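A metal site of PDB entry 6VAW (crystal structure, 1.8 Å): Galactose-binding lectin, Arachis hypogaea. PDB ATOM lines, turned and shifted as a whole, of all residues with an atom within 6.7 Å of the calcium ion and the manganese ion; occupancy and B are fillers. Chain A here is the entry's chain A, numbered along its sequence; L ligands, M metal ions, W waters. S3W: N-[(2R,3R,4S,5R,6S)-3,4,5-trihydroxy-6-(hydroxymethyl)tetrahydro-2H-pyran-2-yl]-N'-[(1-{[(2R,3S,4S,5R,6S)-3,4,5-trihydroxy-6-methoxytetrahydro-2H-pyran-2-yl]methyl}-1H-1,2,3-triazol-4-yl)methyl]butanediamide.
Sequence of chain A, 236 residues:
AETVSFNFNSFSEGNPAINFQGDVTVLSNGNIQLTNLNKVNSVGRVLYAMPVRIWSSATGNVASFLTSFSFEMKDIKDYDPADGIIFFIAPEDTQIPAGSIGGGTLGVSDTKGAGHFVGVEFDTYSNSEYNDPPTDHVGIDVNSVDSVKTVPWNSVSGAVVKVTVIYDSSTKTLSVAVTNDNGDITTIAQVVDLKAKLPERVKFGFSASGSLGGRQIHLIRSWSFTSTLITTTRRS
An oxygen (O3) of the ligand is in hydrogen-bond range of the side-chain amide nitrogen (ND2) of Asn 127 (2.8 Å).
An oxygen (O3) of the ligand sits at hydrogen-bond distance from the backbone NH of Gly 104 (3.0 Å).
An oxygen (O4) of the ligand sits at hydrogen-bond distance from the side-chain carboxylate (OD1) of Asp 83.
OE1 of Glu 121 sits close to OD2 of Asp 141, at 2.7 Å.
The backbone NH (N) of Glu 121 is in hydrogen-bond range of the backbone carbonyl oxygen (O) of Gly 139, at 2.9 Å.
The side-chain hydroxyl (OG) of Ser 126 sits at hydrogen-bond distance from the backbone carbonyl oxygen (O) of Asp 132.
Of the 23 residues printed, 4 come within 4 Å of the manganese ion.
The calcium ion is bound by the backbone carbonyl oxygen (O) of Tyr 125, water W3, the side-chain carboxylate (OD2) of Asp 132, water W1, the side-chain amide oxygen (OD1) of Asn 127, the side-chain carboxylate (OD1) of Asp 123 and the side-chain carboxylate (OD2) of Asp 123.
The side-chain carboxylate (OD2) of Asp 123 is bound to the manganese ion, 2.1 Å away.
The manganese ion is bound by NE2 of His 137.
OE2 of Glu 121 binds the manganese ion, at 2.1 Å.
The side-chain carboxylate (OD1) of Asp 132 binds the manganese ion (2.2 Å).
The manganese ion is bound by water W4 (2.3 Å).
Water W2 is bound to the manganese ion.
Water W2 lies within hydrogen-bond range of O of Val 145 and OE1 of Glu 121.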
ATOM      1  N   ASP A  83      35.577  -8.908  29.715  1.00  0.00           N
ATOM      2  CA  ASP A  83      34.126  -8.763  29.538  1.00  0.00           C
ATOM      3  C   ASP A  83      33.646  -8.342  28.136  1.00  0.00           C
ATOM      4  O   ASP A  83      32.441  -8.417  27.889  1.00  0.00           O
ATOM      5  CB  ASP A  83      33.593  -7.774  30.534  1.00  0.00           C
ATOM      6  CG  ASP A  83      33.330  -8.444  31.847  1.00  0.00           C
ATOM      7  OD1 ASP A  83      34.284  -8.531  32.667  1.00  0.00           O
ATOM      8  OD2 ASP A  83      32.221  -8.994  32.017  1.00  0.00           O
ATOM      9  N   GLY A 103      34.507  -4.898  34.750  1.00  0.00           N
ATOM     10  CA  GLY A 103      33.554  -5.976  34.522  1.00  0.00           C
ATOM     11  C   GLY A 103      32.532  -5.685  33.433  1.00  0.00           C
ATOM     12  O   GLY A 103      32.897  -5.257  32.329  1.00  0.00           O
ATOM     13  N   GLY A 104      31.259  -5.891  33.753  1.00  0.00           N
ATOM     14  CA  GLY A 104      30.116  -5.707  32.865  1.00  0.00           C
ATOM     15  C   GLY A 104      29.833  -4.255  32.493  1.00  0.00           C
ATOM     16  O   GLY A 104      29.016  -4.006  31.601  1.00  0.00           O
ATOM     17  N   THR A 105      30.458  -3.300  33.217  1.00  0.00           N
ATOM     18  CA  THR A 105      30.297  -1.870  32.962  1.00  0.00           C
ATOM     19  C   THR A 105      31.009  -1.458  31.656  1.00  0.00           C
ATOM     20  O   THR A 105      30.810  -0.332  31.206  1.00  0.00           O
ATOM     21  CB  THR A 105      30.783  -0.991  34.151  1.00  0.00           C
ATOM     22  OG1 THR A 105      32.225  -0.870  34.139  1.00  0.00           O
ATOM     23  CG2 THR A 105      30.252  -1.432  35.491  1.00  0.00           C
ATOM     24  N   LEU A 106      31.944  -2.312  31.152  1.00  0.00           N
ATOM     25  CA  LEU A 106      32.775  -2.152  29.930  1.00  0.00           C
ATOM     26  C   LEU A 106      33.633  -0.852  29.947  1.00  0.00           C
ATOM     27  O   LEU A 106      34.106  -0.408  28.886  1.00  0.00           O
ATOM     28  CB  LEU A 106      31.883  -2.224  28.654  1.00  0.00           C
ATOM     29  CG  LEU A 106      31.058  -3.499  28.477  1.00  0.00           C
ATOM     30  CD1 LEU A 106      30.078  -3.361  27.293  1.00  0.00           C
ATOM     31  CD2 LEU A 106      31.954  -4.753  28.344  1.00  0.00           C
ATOM     32  N   GLU A 121      28.445  -2.453  21.649  1.00  0.00           N
ATOM     33  CA  GLU A 121      29.192  -3.395  22.492  1.00  0.00           C
ATOM     34  C   GLU A 121      29.289  -4.770  21.863  1.00  0.00           C
ATOM     35  O   GLU A 121      28.361  -5.250  21.204  1.00  0.00           O
ATOM     36  CB  GLU A 121      28.585  -3.523  23.891  1.00  0.00           C
ATOM     37  CG  GLU A 121      27.121  -3.960  23.859  1.00  0.00           C
ATOM     38  CD  GLU A 121      26.613  -4.344  25.222  1.00  0.00           C
ATOM     39  OE1 GLU A 121      26.556  -3.445  26.077  1.00  0.00           O
ATOM     40  OE2 GLU A 121      26.230  -5.513  25.425  1.00  0.00           O
ATOM     41  N   ASP A 123      29.889  -7.907  23.622  1.00  0.00           N
ATOM     42  CA  ASP A 123      29.769  -8.407  24.984  1.00  0.00           C
ATOM     43  C   ASP A 123      29.933  -9.914  25.081  1.00  0.00           C
ATOM     44  O   ASP A 123      29.194 -10.669  24.461  1.00  0.00           O
ATOM     45  CB  ASP A 123      28.414  -7.962  25.517  1.00  0.00           C
ATOM     46  CG  ASP A 123      28.312  -8.011  27.006  1.00  0.00           C
ATOM     47  OD1 ASP A 123      29.239  -8.559  27.650  1.00  0.00           O
ATOM     48  OD2 ASP A 123      27.342  -7.464  27.546  1.00  0.00           O
ATOM     49  N   THR A 124      30.936 -10.352  25.880  1.00  0.00           N
ATOM     50  CA  THR A 124      31.295 -11.767  25.994  1.00  0.00           C
ATOM     51  C   THR A 124      30.937 -12.401  27.360  1.00  0.00           C
ATOM     52  O   THR A 124      31.314 -13.552  27.614  1.00  0.00           O
ATOM     53  CB  THR A 124      32.783 -11.964  25.680  1.00  0.00           C
ATOM     54  OG1 THR A 124      33.583 -11.383  26.704  1.00  0.00           O
ATOM     55  CG2 THR A 124      33.182 -11.385  24.330  1.00  0.00           C
ATOM     56  N   TYR A 125      30.152 -11.691  28.206  1.00  0.00           N
ATOM     57  CA  TYR A 125      29.737 -12.205  29.528  1.00  0.00           C
ATOM     58  C   TYR A 125      28.342 -11.680  29.872  1.00  0.00           C
ATOM     59  O   TYR A 125      28.083 -10.474  29.789  1.00  0.00           O
ATOM     60  CB  TYR A 125      30.765 -11.842  30.622  1.00  0.00           C
ATOM     61  CG  TYR A 125      30.402 -12.465  31.961  1.00  0.00           C
ATOM     62  CD1 TYR A 125      29.507 -11.834  32.830  1.00  0.00           C
ATOM     63  CD2 TYR A 125      30.908 -13.704  32.339  1.00  0.00           C
ATOM     64  CE1 TYR A 125      29.098 -12.440  34.012  1.00  0.00           C
ATOM     65  CE2 TYR A 125      30.552 -14.296  33.546  1.00  0.00           C
ATOM     66  CZ  TYR A 125      29.651 -13.654  34.388  1.00  0.00           C
ATOM     67  OH  TYR A 125      29.307 -14.230  35.583  1.00  0.00           O
ATOM     68  N   SER A 126      27.449 -12.582  30.298  1.00  0.00           N
ATOM     69  CA  SER A 126      26.067 -12.247  30.629  1.00  0.00           C
ATOM     70  C   SER A 126      25.923 -11.760  32.069  1.00  0.00           C
ATOM     71  O   SER A 126      25.990 -12.554  32.998  1.00  0.00           O
ATOM     72  CB  SER A 126      25.151 -13.443  30.380  1.00  0.00           C
ATOM     73  OG  SER A 126      23.798 -13.105  30.599  1.00  0.00           O
ATOM     74  N   ASN A 127      25.746 -10.433  32.237  1.00  0.00           N
ATOM     75  CA  ASN A 127      25.559  -9.783  33.526  1.00  0.00           C
ATOM     76  C   ASN A 127      24.068  -9.637  33.763  1.00  0.00           C
ATOM     77  O   ASN A 127      23.416  -8.815  33.115  1.00  0.00           O
ATOM     78  CB  ASN A 127      26.263  -8.432  33.560  1.00  0.00           C
ATOM     79  CG  ASN A 127      27.739  -8.529  33.383  1.00  0.00           C
ATOM     80  OD1 ASN A 127      28.251  -8.728  32.275  1.00  0.00           O
ATOM     81  ND2 ASN A 127      28.471  -8.458  34.472  1.00  0.00           N
ATOM     82  N   TYR A 130      22.544  -6.245  34.483  1.00  0.00           N
ATOM     83  CA  TYR A 130      22.393  -5.337  33.324  1.00  0.00           C
ATOM     84  C   TYR A 130      21.466  -5.904  32.270  1.00  0.00           C
ATOM     85  O   TYR A 130      21.463  -5.420  31.133  1.00  0.00           O
ATOM     86  CB  TYR A 130      23.771  -5.025  32.717  1.00  0.00           C
ATOM     87  CG  TYR A 130      24.746  -4.458  33.723  1.00  0.00           C
ATOM     88  CD1 TYR A 130      24.368  -3.427  34.587  1.00  0.00           C
ATOM     89  CD2 TYR A 130      26.060  -4.905  33.776  1.00  0.00           C
ATOM     90  CE1 TYR A 130      25.261  -2.900  35.509  1.00  0.00           C
ATOM     91  CE2 TYR A 130      26.953  -4.406  34.724  1.00  0.00           C
ATOM     92  CZ  TYR A 130      26.552  -3.397  35.593  1.00  0.00           C
ATOM     93  OH  TYR A 130      27.416  -2.865  36.509  1.00  0.00           O
ATOM     94  N   ASN A 131      20.681  -6.916  32.653  1.00  0.00           N
ATOM     95  CA  ASN A 131      19.698  -7.633  31.850  1.00  0.00           C
ATOM     96  C   ASN A 131      20.297  -8.137  30.514  1.00  0.00           C
ATOM     97  O   ASN A 131      19.636  -8.067  29.473  1.00  0.00           O
ATOM     98  CB  ASN A 131      18.427  -6.780  31.617  1.00  0.00           C
ATOM     99  CG  ASN A 131      17.644  -6.535  32.889  1.00  0.00           C
ATOM    100  OD1 ASN A 131      17.282  -7.462  33.621  1.00  0.00           O
ATOM    101  ND2 ASN A 131      17.355  -5.274  33.190  1.00  0.00           N
ATOM    102  N   ASP A 132      21.538  -8.661  30.568  1.00  0.00           N
ATOM    103  CA  ASP A 132      22.217  -9.187  29.382  1.00  0.00           C
ATOM    104  C   ASP A 132      21.494 -10.410  28.842  1.00  0.00           C
ATOM    105  O   ASP A 132      21.033 -11.214  29.643  1.00  0.00           O
ATOM    106  CB  ASP A 132      23.666  -9.580  29.717  1.00  0.00           C
ATOM    107  CG  ASP A 132      24.707  -8.492  29.515  1.00  0.00           C
ATOM    108  OD1 ASP A 132      24.454  -7.571  28.699  1.00  0.00           O
ATOM    109  OD2 ASP A 132      25.772  -8.563  30.160  1.00  0.00           O
ATOM    110  N   PRO A 133      21.486 -10.635  27.508  1.00  0.00           N
ATOM    111  CA  PRO A 133      20.909 -11.898  26.994  1.00  0.00           C
ATOM    112  C   PRO A 133      21.789 -13.098  27.424  1.00  0.00           C
ATOM    113  O   PRO A 133      22.914 -12.879  27.874  1.00  0.00           O
ATOM    114  CB  PRO A 133      20.860 -11.694  25.469  1.00  0.00           C
ATOM    115  CG  PRO A 133      21.849 -10.627  25.189  1.00  0.00           C
ATOM    116  CD  PRO A 133      22.014  -9.786  26.414  1.00  0.00           C
ATOM    117  N   HIS A 137      26.870 -11.347  22.574  1.00  0.00           N
ATOM    118  CA  HIS A 137      25.972 -10.521  21.784  1.00  0.00           C
ATOM    119  C   HIS A 137      26.603  -9.206  21.384  1.00  0.00           C
ATOM    120  O   HIS A 137      27.562  -8.740  22.020  1.00  0.00           O
ATOM    121  CB  HIS A 137      24.675 -10.227  22.584  1.00  0.00           C
ATOM    122  CG  HIS A 137      24.928  -9.651  23.942  1.00  0.00           C
ATOM    123  ND1 HIS A 137      25.276 -10.458  25.032  1.00  0.00           N
ATOM    124  CD2 HIS A 137      24.846  -8.371  24.372  1.00  0.00           C
ATOM    125  CE1 HIS A 137      25.416  -9.640  26.058  1.00  0.00           C
ATOM    126  NE2 HIS A 137      25.164  -8.377  25.714  1.00  0.00           N
ATOM    127  N   VAL A 138      26.021  -8.596  20.352  1.00  0.00           N
ATOM    128  CA  VAL A 138      26.337  -7.245  19.915  1.00  0.00           C
ATOM    129  C   VAL A 138      25.159  -6.424  20.375  1.00  0.00           C
ATOM    130  O   VAL A 138      24.009  -6.838  20.202  1.00  0.00           O
ATOM    131  CB  VAL A 138      26.627  -7.109  18.401  1.00  0.00           C
ATOM    132  CG1 VAL A 138      27.000  -5.663  18.041  1.00  0.00           C
ATOM    133  CG2 VAL A 138      27.736  -8.060  17.957  1.00  0.00           C
ATOM    134  N   GLY A 139      25.419  -5.290  21.004  1.00  0.00           N
ATOM    135  CA  GLY A 139      24.351  -4.448  21.516  1.00  0.00           C
ATOM    136  C   GLY A 139      24.509  -3.007  21.146  1.00  0.00           C
ATOM    137  O   GLY A 139      25.615  -2.551  20.885  1.00  0.00           O
ATOM    138  N   ASP A 141      23.841   0.624  22.711  1.00  0.00           N
ATOM    139  CA  ASP A 141      23.724   1.224  24.053  1.00  0.00           C
ATOM    140  C   ASP A 141      23.529   2.698  24.014  1.00  0.00           C
ATOM    141  O   ASP A 141      24.268   3.399  23.362  1.00  0.00           O
ATOM    142  CB  ASP A 141      25.005   0.967  24.847  1.00  0.00           C
ATOM    143  CG  ASP A 141      25.265  -0.478  25.176  1.00  0.00           C
ATOM    144  OD1 ASP A 141      24.365  -1.310  24.948  1.00  0.00           O
ATOM    145  OD2 ASP A 141      26.329  -0.758  25.741  1.00  0.00           O
ATOM    146  N   VAL A 145      24.562   0.239  29.846  1.00  0.00           N
ATOM    147  CA  VAL A 145      25.033  -1.066  29.393  1.00  0.00           C
ATOM    148  C   VAL A 145      23.860  -2.071  29.462  1.00  0.00           C
ATOM    149  O   VAL A 145      24.032  -3.267  29.196  1.00  0.00           O
ATOM    150  CB  VAL A 145      26.322  -1.590  30.100  1.00  0.00           C
ATOM    151  CG1 VAL A 145      27.539  -0.757  29.702  1.00  0.00           C
ATOM    152  CG2 VAL A 145      26.162  -1.639  31.615  1.00  0.00           C
ATOM    153  N   ASP A 146      22.638  -1.585  29.790  1.00  0.00           N
ATOM    154  CA  ASP A 146      21.384  -2.329  29.637  1.00  0.00           C
ATOM    155  C   ASP A 146      20.921  -1.901  28.227  1.00  0.00           C
ATOM    156  O   ASP A 146      20.281  -0.871  28.058  1.00  0.00           O
ATOM    157  CB  ASP A 146      20.348  -2.012  30.735  1.00  0.00           C
ATOM    158  CG  ASP A 146      19.102  -2.903  30.698  1.00  0.00           C
ATOM    159  OD1 ASP A 146      18.758  -3.418  29.600  1.00  0.00           O
ATOM    160  OD2 ASP A 146      18.468  -3.088  31.766  1.00  0.00           O
ATOM    161  N   SER A 147      21.380  -2.637  27.217  1.00  0.00           N
ATOM    162  CA  SER A 147      21.201  -2.261  25.814  1.00  0.00           C
ATOM    163  C   SER A 147      19.749  -1.999  25.385  1.00  0.00           C
ATOM    164  O   SER A 147      18.805  -2.670  25.801  1.00  0.00           O
ATOM    165  CB  SER A 147      21.805  -3.304  24.895  1.00  0.00           C
ATOM    166  OG  SER A 147      23.137  -3.587  25.252  1.00  0.00           O
ATOM    167  N   THR A 150      19.827  -5.866  21.292  1.00  0.00           N
ATOM    168  CA  THR A 150      20.934  -6.809  21.153  1.00  0.00           C
ATOM    169  C   THR A 150      20.621  -7.813  20.048  1.00  0.00           C
ATOM    170  O   THR A 150      19.453  -8.026  19.687  1.00  0.00           O
ATOM    171  CB  THR A 150      21.294  -7.595  22.459  1.00  0.00           C
ATOM    172  OG1 THR A 150      20.249  -8.498  22.788  1.00  0.00           O
ATOM    173  CG2 THR A 150      21.672  -6.698  23.634  1.00  0.00           C
HETATM  174  N1  S3W L   1      31.942 -10.657  38.978  1.00  0.00           N
HETATM  175  N2  S3W L   1      33.907 -13.745  42.700  1.00  0.00           N
HETATM  176  C11 S3W L   1      35.239 -14.300  42.721  1.00  0.00           C
HETATM  177  C4  S3W L   1      32.517 -10.909  34.788  1.00  0.00           C
HETATM  178  C3  S3W L   1      31.396 -10.011  35.309  1.00  0.00           C
HETATM  179  C5  S3W L   1      32.694 -12.106  35.728  1.00  0.00           C
HETATM  180  C1  S3W L   1      31.738 -10.951  37.593  1.00  0.00           C
HETATM  181  C2  S3W L   1      31.619  -9.665  36.778  1.00  0.00           C
HETATM  182  C6  S3W L   1      33.645 -13.221  35.383  1.00  0.00           C
HETATM  183  C7  S3W L   1      31.548 -11.465  39.969  1.00  0.00           C
HETATM  184  C8  S3W L   1      31.821 -10.969  41.373  1.00  0.00           C
HETATM  185  C9  S3W L   1      32.201 -12.074  42.349  1.00  0.00           C
HETATM  186  C10 S3W L   1      33.627 -12.539  42.197  1.00  0.00           C
HETATM  187  O5  S3W L   1      32.839 -11.728  37.109  1.00  0.00           O
HETATM  188  O2  S3W L   1      30.531  -8.893  37.260  1.00  0.00           O
HETATM  189  O3  S3W L   1      31.278  -8.835  34.525  1.00  0.00           O
HETATM  190  O4  S3W L   1      33.723 -10.170  34.658  1.00  0.00           O
HETATM  191  O6  S3W L   1      33.189 -14.462  35.918  1.00  0.00           O
HETATM  192  O10 S3W L   1      34.479 -11.827  41.670  1.00  0.00           O
HETATM  193  O7  S3W L   1      30.967 -12.526  39.769  1.00  0.00           O
HETATM  194 CA    CA M   1      28.106  -8.329  29.840  1.00  0.00          CA
HETATM  195 MN    MN M   2      25.486  -6.748  26.977  1.00  0.00          MN
HETATM  196  O   HOH W   1      27.771  -5.981  30.231  1.00  0.00           O
HETATM  197  O   HOH W   2      26.014  -4.753  28.369  1.00  0.00           O
HETATM  198  O   HOH W   3      30.380  -8.113  30.051  1.00  0.00           O
HETATM  199  O   HOH W   4      23.383  -6.006  26.507  1.00  0.00           O
